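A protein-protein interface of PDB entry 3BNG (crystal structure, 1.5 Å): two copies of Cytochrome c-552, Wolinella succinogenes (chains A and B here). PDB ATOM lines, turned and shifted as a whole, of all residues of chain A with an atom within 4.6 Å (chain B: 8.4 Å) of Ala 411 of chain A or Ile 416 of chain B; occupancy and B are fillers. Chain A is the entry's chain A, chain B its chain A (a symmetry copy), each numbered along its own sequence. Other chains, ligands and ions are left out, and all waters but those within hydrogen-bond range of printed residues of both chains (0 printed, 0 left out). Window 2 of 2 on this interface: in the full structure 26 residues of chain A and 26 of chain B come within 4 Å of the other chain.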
ATOM      1  N   VAL A 407      19.781  20.754 -17.732  1.00  0.00           N
ATOM      2  CA  VAL A 407      20.947  20.218 -18.451  1.00  0.00           C
ATOM      3  C   VAL A 407      22.045  21.271 -18.414  1.00  0.00           C
ATOM      4  O   VAL A 407      23.217  20.942 -18.196  1.00  0.00           O
ATOM      5  CB  VAL A 407      20.672  19.840 -19.923  1.00  0.00           C
ATOM      6  CG1 VAL A 407      21.962  19.329 -20.607  1.00  0.00           C
ATOM      7  CG2 VAL A 407      19.572  18.768 -20.022  1.00  0.00           C
ATOM      8  N   LYS A 408      21.663  22.533 -18.589  1.00  0.00           N
ATOM      9  CA  LYS A 408      22.666  23.603 -18.635  1.00  0.00           C
ATOM     10  C   LYS A 408      23.263  23.898 -17.260  1.00  0.00           C
ATOM     11  O   LYS A 408      24.457  24.164 -17.160  1.00  0.00           O
ATOM     12  CB  LYS A 408      22.116  24.847 -19.329  1.00  0.00           C
ATOM     13  CG  LYS A 408      21.585  24.504 -20.706  1.00  0.00           C
ATOM     14  CD  LYS A 408      21.291  25.714 -21.541  1.00  0.00           C
ATOM     15  CE  LYS A 408      20.354  25.323 -22.659  1.00  0.00           C
ATOM     16  NZ  LYS A 408      19.142  24.723 -22.037  1.00  0.00           N
ATOM     17  N   VAL A 409      22.453  23.821 -16.204  1.00  0.00           N
ATOM     18  CA  VAL A 409      23.006  23.944 -14.846  1.00  0.00           C
ATOM     19  C   VAL A 409      23.950  22.781 -14.552  1.00  0.00           C
ATOM     20  O   VAL A 409      25.068  23.011 -14.085  1.00  0.00           O
ATOM     21  CB  VAL A 409      21.907  24.073 -13.763  1.00  0.00           C
ATOM     22  CG1 VAL A 409      22.528  24.191 -12.383  1.00  0.00           C
ATOM     23  CG2 VAL A 409      21.060  25.328 -14.075  1.00  0.00           C
ATOM     24  N   LEU A 410      23.528  21.540 -14.836  1.00  0.00           N
ATOM     25  CA  LEU A 410      24.405  20.393 -14.615  1.00  0.00           C
ATOM     26  C   LEU A 410      25.715  20.602 -15.383  1.00  0.00           C
ATOM     27  O   LEU A 410      26.788  20.402 -14.809  1.00  0.00           O
ATOM     28  CB  LEU A 410      23.722  19.082 -14.996  1.00  0.00           C
ATOM     29  CG  LEU A 410      22.583  18.723 -14.052  1.00  0.00           C
ATOM     30  CD1 LEU A 410      21.788  17.604 -14.717  1.00  0.00           C
ATOM     31  CD2 LEU A 410      23.144  18.244 -12.715  1.00  0.00           C
ATOM     32  N   ALA A 411      25.627  21.055 -16.630  1.00  0.00           N
ATOM     33  CA  ALA A 411      26.843  21.258 -17.455  1.00  0.00           C
ATOM     34  C   ALA A 411      27.776  22.266 -16.813  1.00  0.00           C
ATOM     35  O   ALA A 411      29.006  22.072 -16.803  1.00  0.00           O
ATOM     36  CB  ALA A 411      26.486  21.720 -18.844  1.00  0.00           C
ATOM     37  N   LYS A 412      27.190  23.340 -16.290  1.00  0.00           N
ATOM     38  CA  LYS A 412      27.959  24.395 -15.644  1.00  0.00           C
ATOM     39  C   LYS A 412      28.836  23.809 -14.543  1.00  0.00           C
ATOM     40  O   LYS A 412      30.009  24.184 -14.411  1.00  0.00           O
ATOM     41  CB  LYS A 412      27.031  25.464 -15.070  1.00  0.00           C
ATOM     42  CG  LYS A 412      27.782  26.556 -14.343  1.00  0.00           C
ATOM     43  CD  LYS A 412      26.898  27.583 -13.691  1.00  0.00           C
ATOM     44  CE  LYS A 412      27.753  28.766 -13.309  1.00  0.00           C
ATOM     45  NZ  LYS A 412      27.619  29.082 -11.889  1.00  0.00           N
ATOM     46  N   TYR A 413      28.272  22.860 -13.798  1.00  0.00           N
ATOM     47  CA  TYR A 413      28.967  22.201 -12.686  1.00  0.00           C
ATOM     48  C   TYR A 413      29.655  20.874 -13.043  1.00  0.00           C
ATOM     49  O   TYR A 413      30.033  20.110 -12.155  1.00  0.00           O
ATOM     50  CB  TYR A 413      27.997  22.044 -11.517  1.00  0.00           C
ATOM     51  CG  TYR A 413      27.653  23.389 -10.952  1.00  0.00           C
ATOM     52  CD1 TYR A 413      28.547  24.042 -10.070  1.00  0.00           C
ATOM     53  CD2 TYR A 413      26.500  24.069 -11.332  1.00  0.00           C
ATOM     54  CE1 TYR A 413      28.270  25.297  -9.561  1.00  0.00           C
ATOM     55  CE2 TYR A 413      26.208  25.323 -10.798  1.00  0.00           C
ATOM     56  CZ  TYR A 413      27.100  25.935  -9.921  1.00  0.00           C
ATOM     57  OH  TYR A 413      26.837  27.190  -9.424  1.00  0.00           O
ATOM     58  N   GLY A 414      29.803  20.604 -14.337  1.00  0.00           N
ATOM     59  CA  GLY A 414      30.634  19.500 -14.836  1.00  0.00           C
ATOM     60  C   GLY A 414      29.921  18.157 -14.891  1.00  0.00           C
ATOM     61  O   GLY A 414      30.565  17.092 -14.984  1.00  0.00           O
ATOM     62  N   ALA A 415      28.586  18.179 -14.852  1.00  0.00           N
ATOM     63  CA  ALA A 415      27.835  16.929 -14.750  1.00  0.00           C
ATOM     64  C   ALA A 415      26.807  16.759 -15.853  1.00  0.00           C
ATOM     65  O   ALA A 415      25.686  16.246 -15.613  1.00  0.00           O
ATOM     66  CB  ALA A 415      27.175  16.831 -13.419  1.00  0.00           C
ATOM     67  N   ILE A 416      27.177  17.157 -17.070  1.00  0.00           N
ATOM     68  CA  ILE A 416      26.198  17.134 -18.158  1.00  0.00           C
ATOM     69  C   ILE A 416      25.682  15.727 -18.467  1.00  0.00           C
ATOM     70  O   ILE A 416      24.540  15.569 -18.907  1.00  0.00           O
ATOM     71  CB  ILE A 416      26.705  17.838 -19.456  1.00  0.00           C
ATOM     72  CG1 ILE A 416      25.509  18.270 -20.322  1.00  0.00           C
ATOM     73  CG2 ILE A 416      27.653  16.940 -20.233  1.00  0.00           C
ATOM     74  CD1 ILE A 416      25.876  19.236 -21.427  1.00  0.00           C
ATOM     75  N   GLU B 343      17.547  23.690 -33.661  1.00  0.00           N
ATOM     76  CA  GLU B 343      18.690  23.300 -32.827  1.00  0.00           C
ATOM     77  C   GLU B 343      19.479  22.202 -33.508  1.00  0.00           C
ATOM     78  O   GLU B 343      20.693  22.170 -33.388  1.00  0.00           O
ATOM     79  CB  GLU B 343      18.228  22.860 -31.456  1.00  0.00           C
ATOM     80  CG  GLU B 343      17.706  24.046 -30.661  1.00  0.00           C
ATOM     81  CD  GLU B 343      16.776  23.673 -29.502  1.00  0.00           C
ATOM     82  OE1 GLU B 343      16.444  22.484 -29.315  1.00  0.00           O
ATOM     83  OE2 GLU B 343      16.341  24.589 -28.768  1.00  0.00           O
ATOM     84  N   LYS B 346      21.544  23.867 -36.170  1.00  0.00           N
ATOM     85  CA  LYS B 346      22.689  24.545 -35.589  1.00  0.00           C
ATOM     86  C   LYS B 346      23.771  23.524 -35.208  1.00  0.00           C
ATOM     87  O   LYS B 346      24.944  23.734 -35.480  1.00  0.00           O
ATOM     88  CB  LYS B 346      22.264  25.356 -34.372  1.00  0.00           C
ATOM     89  CG  LYS B 346      23.431  25.978 -33.554  1.00  0.00           C
ATOM     90  CD  LYS B 346      24.093  27.081 -34.349  1.00  0.00           C
ATOM     91  CE  LYS B 346      25.042  27.834 -33.427  1.00  0.00           C
ATOM     92  NZ  LYS B 346      25.712  28.930 -34.144  1.00  0.00           N
ATOM     93  N   LEU B 350      27.700  23.200 -36.686  1.00  0.00           N
ATOM     94  CA  LEU B 350      28.870  23.152 -35.812  1.00  0.00           C
ATOM     95  C   LEU B 350      29.720  21.909 -36.045  1.00  0.00           C
ATOM     96  O   LEU B 350      30.841  21.826 -35.544  1.00  0.00           O
ATOM     97  CB  LEU B 350      28.451  23.248 -34.346  1.00  0.00           C
ATOM     98  CG  LEU B 350      27.843  24.570 -33.866  1.00  0.00           C
ATOM     99  CD1 LEU B 350      27.183  24.364 -32.538  1.00  0.00           C
ATOM    100  CD2 LEU B 350      28.896  25.719 -33.801  1.00  0.00           C
ATOM    101  N   LEU B 406      19.532  17.360 -27.528  1.00  0.00           N
ATOM    102  CA  LEU B 406      20.210  18.403 -28.287  1.00  0.00           C
ATOM    103  C   LEU B 406      21.051  19.336 -27.442  1.00  0.00           C
ATOM    104  O   LEU B 406      22.086  19.836 -27.915  1.00  0.00           O
ATOM    105  CB  LEU B 406      19.233  19.257 -29.106  1.00  0.00           C
ATOM    106  CG  LEU B 406      18.804  18.642 -30.431  1.00  0.00           C
ATOM    107  CD1 LEU B 406      17.394  19.091 -30.866  1.00  0.00           C
ATOM    108  CD2 LEU B 406      19.876  18.806 -31.541  1.00  0.00           C
ATOM    109  N   VAL B 407      20.602  19.631 -26.211  1.00  0.00           N
ATOM    110  CA  VAL B 407      21.381  20.537 -25.353  1.00  0.00           C
ATOM    111  C   VAL B 407      22.781  19.959 -25.211  1.00  0.00           C
ATOM    112  O   VAL B 407      23.771  20.699 -25.274  1.00  0.00           O
ATOM    113  CB  VAL B 407      20.787  20.749 -23.944  1.00  0.00           C
ATOM    114  CG1 VAL B 407      21.694  21.678 -23.102  1.00  0.00           C
ATOM    115  CG2 VAL B 407      19.370  21.343 -24.025  1.00  0.00           C
ATOM    116  N   LYS B 408      22.867  18.640 -25.058  1.00  0.00           N
ATOM    117  CA  LYS B 408      24.175  18.009 -24.846  1.00  0.00           C
ATOM    118  C   LYS B 408      25.021  17.988 -26.117  1.00  0.00           C
ATOM    119  O   LYS B 408      26.231  18.180 -26.045  1.00  0.00           O
ATOM    120  CB  LYS B 408      24.027  16.632 -24.202  1.00  0.00           C
ATOM    121  CG  LYS B 408      23.223  16.722 -22.921  1.00  0.00           C
ATOM    122  CD  LYS B 408      23.278  15.467 -22.103  1.00  0.00           C
ATOM    123  CE  LYS B 408      22.120  15.460 -21.135  1.00  0.00           C
ATOM    124  NZ  LYS B 408      20.870  15.592 -21.934  1.00  0.00           N
ATOM    125  N   VAL B 409      24.392  17.792 -27.277  1.00  0.00           N
ATOM    126  CA  VAL B 409      25.134  17.916 -28.542  1.00  0.00           C
ATOM    127  C   VAL B 409      25.619  19.350 -28.733  1.00  0.00           C
ATOM    128  O   VAL B 409      26.796  19.556 -29.036  1.00  0.00           O
ATOM    129  CB  VAL B 409      24.318  17.422 -29.762  1.00  0.00           C
ATOM    130  CG1 VAL B 409      25.122  17.575 -31.039  1.00  0.00           C
ATOM    131  CG2 VAL B 409      23.952  15.937 -29.537  1.00  0.00           C
ATOM    132  N   LEU B 410      24.738  20.343 -28.543  1.00  0.00           N
ATOM    133  CA  LEU B 410      25.157  21.736 -28.671  1.00  0.00           C
ATOM    134  C   LEU B 410      26.334  22.000 -27.725  1.00  0.00           C
ATOM    135  O   LEU B 410      27.328  22.593 -28.151  1.00  0.00           O
ATOM    136  CB  LEU B 410      23.997  22.697 -28.422  1.00  0.00           C
ATOM    137  CG  LEU B 410      22.947  22.640 -29.523  1.00  0.00           C
ATOM    138  CD1 LEU B 410      21.715  23.374 -29.003  1.00  0.00           C
ATOM    139  CD2 LEU B 410      23.473  23.326 -30.782  1.00  0.00           C
ATOM    140  N   ALA B 411      26.247  21.514 -26.490  1.00  0.00           N
ATOM    141  CA  ALA B 411      27.326  21.747 -25.501  1.00  0.00           C
ATOM    142  C   ALA B 411      28.642  21.166 -25.982  1.00  0.00           C
ATOM    143  O   ALA B 411      29.705  21.796 -25.828  1.00  0.00           O
ATOM    144  CB  ALA B 411      26.975  21.150 -24.162  1.00  0.00           C
ATOM    145  N   LYS B 412      28.566  19.967 -26.552  1.00  0.00           N
ATOM    146  CA  LYS B 412      29.748  19.283 -27.058  1.00  0.00           C
ATOM    147  C   LYS B 412      30.494  20.177 -28.043  1.00  0.00           C
ATOM    148  O   LYS B 412      31.729  20.260 -28.002  1.00  0.00           O
ATOM    149  CB  LYS B 412      29.363  17.964 -27.726  1.00  0.00           C
ATOM    150  CG  LYS B 412      30.554  17.242 -28.315  1.00  0.00           C
ATOM    151  CD  LYS B 412      30.205  15.980 -29.055  1.00  0.00           C
ATOM    152  CE  LYS B 412      31.476  15.201 -29.284  1.00  0.00           C
ATOM    153  NZ  LYS B 412      31.664  14.895 -30.700  1.00  0.00           N
ATOM    154  N   TYR B 413      29.731  20.874 -28.883  1.00  0.00           N
ATOM    155  CA  TYR B 413      30.283  21.770 -29.905  1.00  0.00           C
ATOM    156  C   TYR B 413      30.382  23.246 -29.492  1.00  0.00           C
ATOM    157  O   TYR B 413      30.574  24.119 -30.339  1.00  0.00           O
ATOM    158  CB  TYR B 413      29.494  21.592 -31.200  1.00  0.00           C
ATOM    159  CG  TYR B 413      29.746  20.230 -31.773  1.00  0.00           C
ATOM    160  CD1 TYR B 413      30.928  19.972 -32.506  1.00  0.00           C
ATOM    161  CD2 TYR B 413      28.880  19.166 -31.537  1.00  0.00           C
ATOM    162  CE1 TYR B 413      31.201  18.716 -33.015  1.00  0.00           C
ATOM    163  CE2 TYR B 413      29.143  17.907 -32.073  1.00  0.00           C
ATOM    164  CZ  TYR B 413      30.307  17.686 -32.803  1.00  0.00           C
ATOM    165  OH  TYR B 413      30.592  16.435 -33.298  1.00  0.00           O
ATOM    166  N   GLY B 414      30.242  23.518 -28.197  1.00  0.00           N
ATOM    167  CA  GLY B 414      30.536  24.836 -27.618  1.00  0.00           C
ATOM    168  C   GLY B 414      29.381  25.824 -27.697  1.00  0.00           C
ATOM    169  O   GLY B 414      29.572  27.048 -27.544  1.00  0.00           O
ATOM    170  N   ALA B 415      28.166  25.317 -27.918  1.00  0.00           N
ATOM    171  CA  ALA B 415      27.032  26.208 -28.156  1.00  0.00           C
ATOM    172  C   ALA B 415      25.871  25.963 -27.209  1.00  0.00           C
ATOM    173  O   ALA B 415      24.685  26.038 -27.614  1.00  0.00           O
ATOM    174  CB  ALA B 415      26.571  26.094 -29.567  1.00  0.00           C
ATOM    175  N   ILE B 416      26.190  25.696 -25.943  1.00  0.00           N
ATOM    176  CA  ILE B 416      25.131  25.331 -25.001  1.00  0.00           C
ATOM    177  C   ILE B 416      24.099  26.445 -24.803  1.00  0.00           C
ATOM    178  O   ILE B 416      22.930  26.163 -24.529  1.00  0.00           O
ATOM    179  CB  ILE B 416      25.675  24.827 -23.628  1.00  0.00           C
ATOM    180  CG1 ILE B 416      24.613  23.966 -22.924  1.00  0.00           C
ATOM    181  CG2 ILE B 416      26.114  25.989 -22.751  1.00  0.00           C
ATOM    182  CD1 ILE B 416      25.151  23.172 -21.753  1.00  0.00           C
ATOM    183  N   ASP B 417      24.532  27.694 -24.965  1.00  0.00           N
ATOM    184  CA  ASP B 417      23.654  28.861 -24.756  1.00  0.00           C
ATOM    185  C   ASP B 417      22.910  29.327 -26.023  1.00  0.00           C
ATOM    186  O   ASP B 417      22.238  30.359 -25.993  1.00  0.00           O
ATOM    187  CB  ASP B 417      24.423  30.021 -24.136  1.00  0.00           C
ATOM    188  CG  ASP B 417      24.931  29.692 -22.753  1.00  0.00           C
ATOM    189  OD1 ASP B 417      24.137  29.128 -21.968  1.00  0.00           O
ATOM    190  OD2 ASP B 417      26.116  29.981 -22.461  1.00  0.00           O
ATOM    191  N   TYR B 418      23.030  28.571 -27.111  1.00  0.00           N
ATOM    192  CA  TYR B 418      22.295  28.852 -28.352  1.00  0.00           C
ATOM    193  C   TYR B 418      20.791  28.983 -28.104  1.00  0.00           C
ATOM    194  O   TYR B 418      20.193  28.183 -27.383  1.00  0.00           O
ATOM    195  CB  TYR B 418      22.549  27.731 -29.364  1.00  0.00           C
ATOM    196  CG  TYR B 418      21.757  27.851 -30.652  1.00  0.00           C
ATOM    197  CD1 TYR B 418      22.072  28.835 -31.607  1.00  0.00           C
ATOM    198  CD2 TYR B 418      20.738  26.946 -30.944  1.00  0.00           C
ATOM    199  CE1 TYR B 418      21.345  28.936 -32.802  1.00  0.00           C
ATOM    200  CE2 TYR B 418      20.027  27.026 -32.128  1.00  0.00           C
ATOM    201  CZ  TYR B 418      20.328  28.009 -33.049  1.00  0.00           C
ATOM    202  OH  TYR B 418      19.585  28.037 -34.209  1.00  0.00           O
ATOM    203  N   VAL B 419      20.188  29.979 -28.738  1.00  0.00           N
ATOM    204  CA  VAL B 419      18.759  30.209 -28.637  1.00  0.00           C
ATOM    205  C   VAL B 419      18.228  30.091 -30.056  1.00  0.00           C
ATOM    206  O   VAL B 419      18.593  30.893 -30.927  1.00  0.00           O
ATOM    207  CB  VAL B 419      18.437  31.614 -28.059  1.00  0.00           C
ATOM    208  CG1 VAL B 419      16.939  31.789 -27.899  1.00  0.00           C
ATOM    209  CG2 VAL B 419      19.115  31.821 -26.716  1.00  0.00           C
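Ala 411 of chain A touches just one residue of chain B: Ile 416.
Of the printed residues of chain A, Val 407 of chain B touches Val 407 (3.4 Å) and Lys 408 (3.7 Å).
Val 409 of chain B touches none of the printed residues of chain A.
Printed residues of chain A within 4 Å of Ala 411 of chain B: Ile 416 (3.5 Å).
Of the printed residues of chain A, Ile 416 of chain B touches Lys 408 (3.3 Å) and Ala 411 (3.5 Å).
The nearest printed residue of chain A that does not touch Ile 416 of chain B is Ile 416 of chain A (4.02 Å).
Val 407 of chain A touches Val 407 of chain B (CG1 to CG1, 3.4 Å).
CG1 of Val 407 of chain A touches CG of Lys 408 of chain B, at 3.7 Å.
Lys 408 of chain A touches Val 407 of chain B.
O of Ile 416 of chain B touches CE of Lys 408 of chain A (3.3 Å).
CB of Ala 411 of chain A touches CD1 of Ile 416 of chain B, 3.5 Å away.
O of Ile 416 of chain A touches CE of Lys 408 of chain B, 3.3 Å away.
CD1 of Ile 416 of chain A touches CB of Ala 411 of chain B, 3.5 Å away.
Val 407 of chain A touches its own counterpart, Val 407 of chain B.
Val 407 of chain A touches Lys 408 of chain B, and with the chains exchanged Lys 408 of chain A touches Val 407 of chain B.
Lys 408 of chain A touches Ile 416 of chain B, and with the chains exchanged Ile 416 of chain A touches Lys 408 of chain B.
Ala 411 of chain A touches Ile 416 of chain B, and with the chains exchanged Ile 416 of chain A touches Ala 411 of chain B.
Positions printed for both chains: 407, 408, 409, 410, 411, 412, 413, 414, 415 and 416.
Of the 10 printed residues of chain A, 4 touch a printed residue of chain B.
Hydrophobic or aromatic side chains of chain A within 4 Å of the printed part of chain B: Val 407, Ala 411 and Ile 416.
Hydrophobic or aromatic side chains of chain B that line the printed part of chain A: Val 407, Ala 411 and Ile 416.
Along chain B the printed residues that touch a printed residue of chain A span positions 407 to 416.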
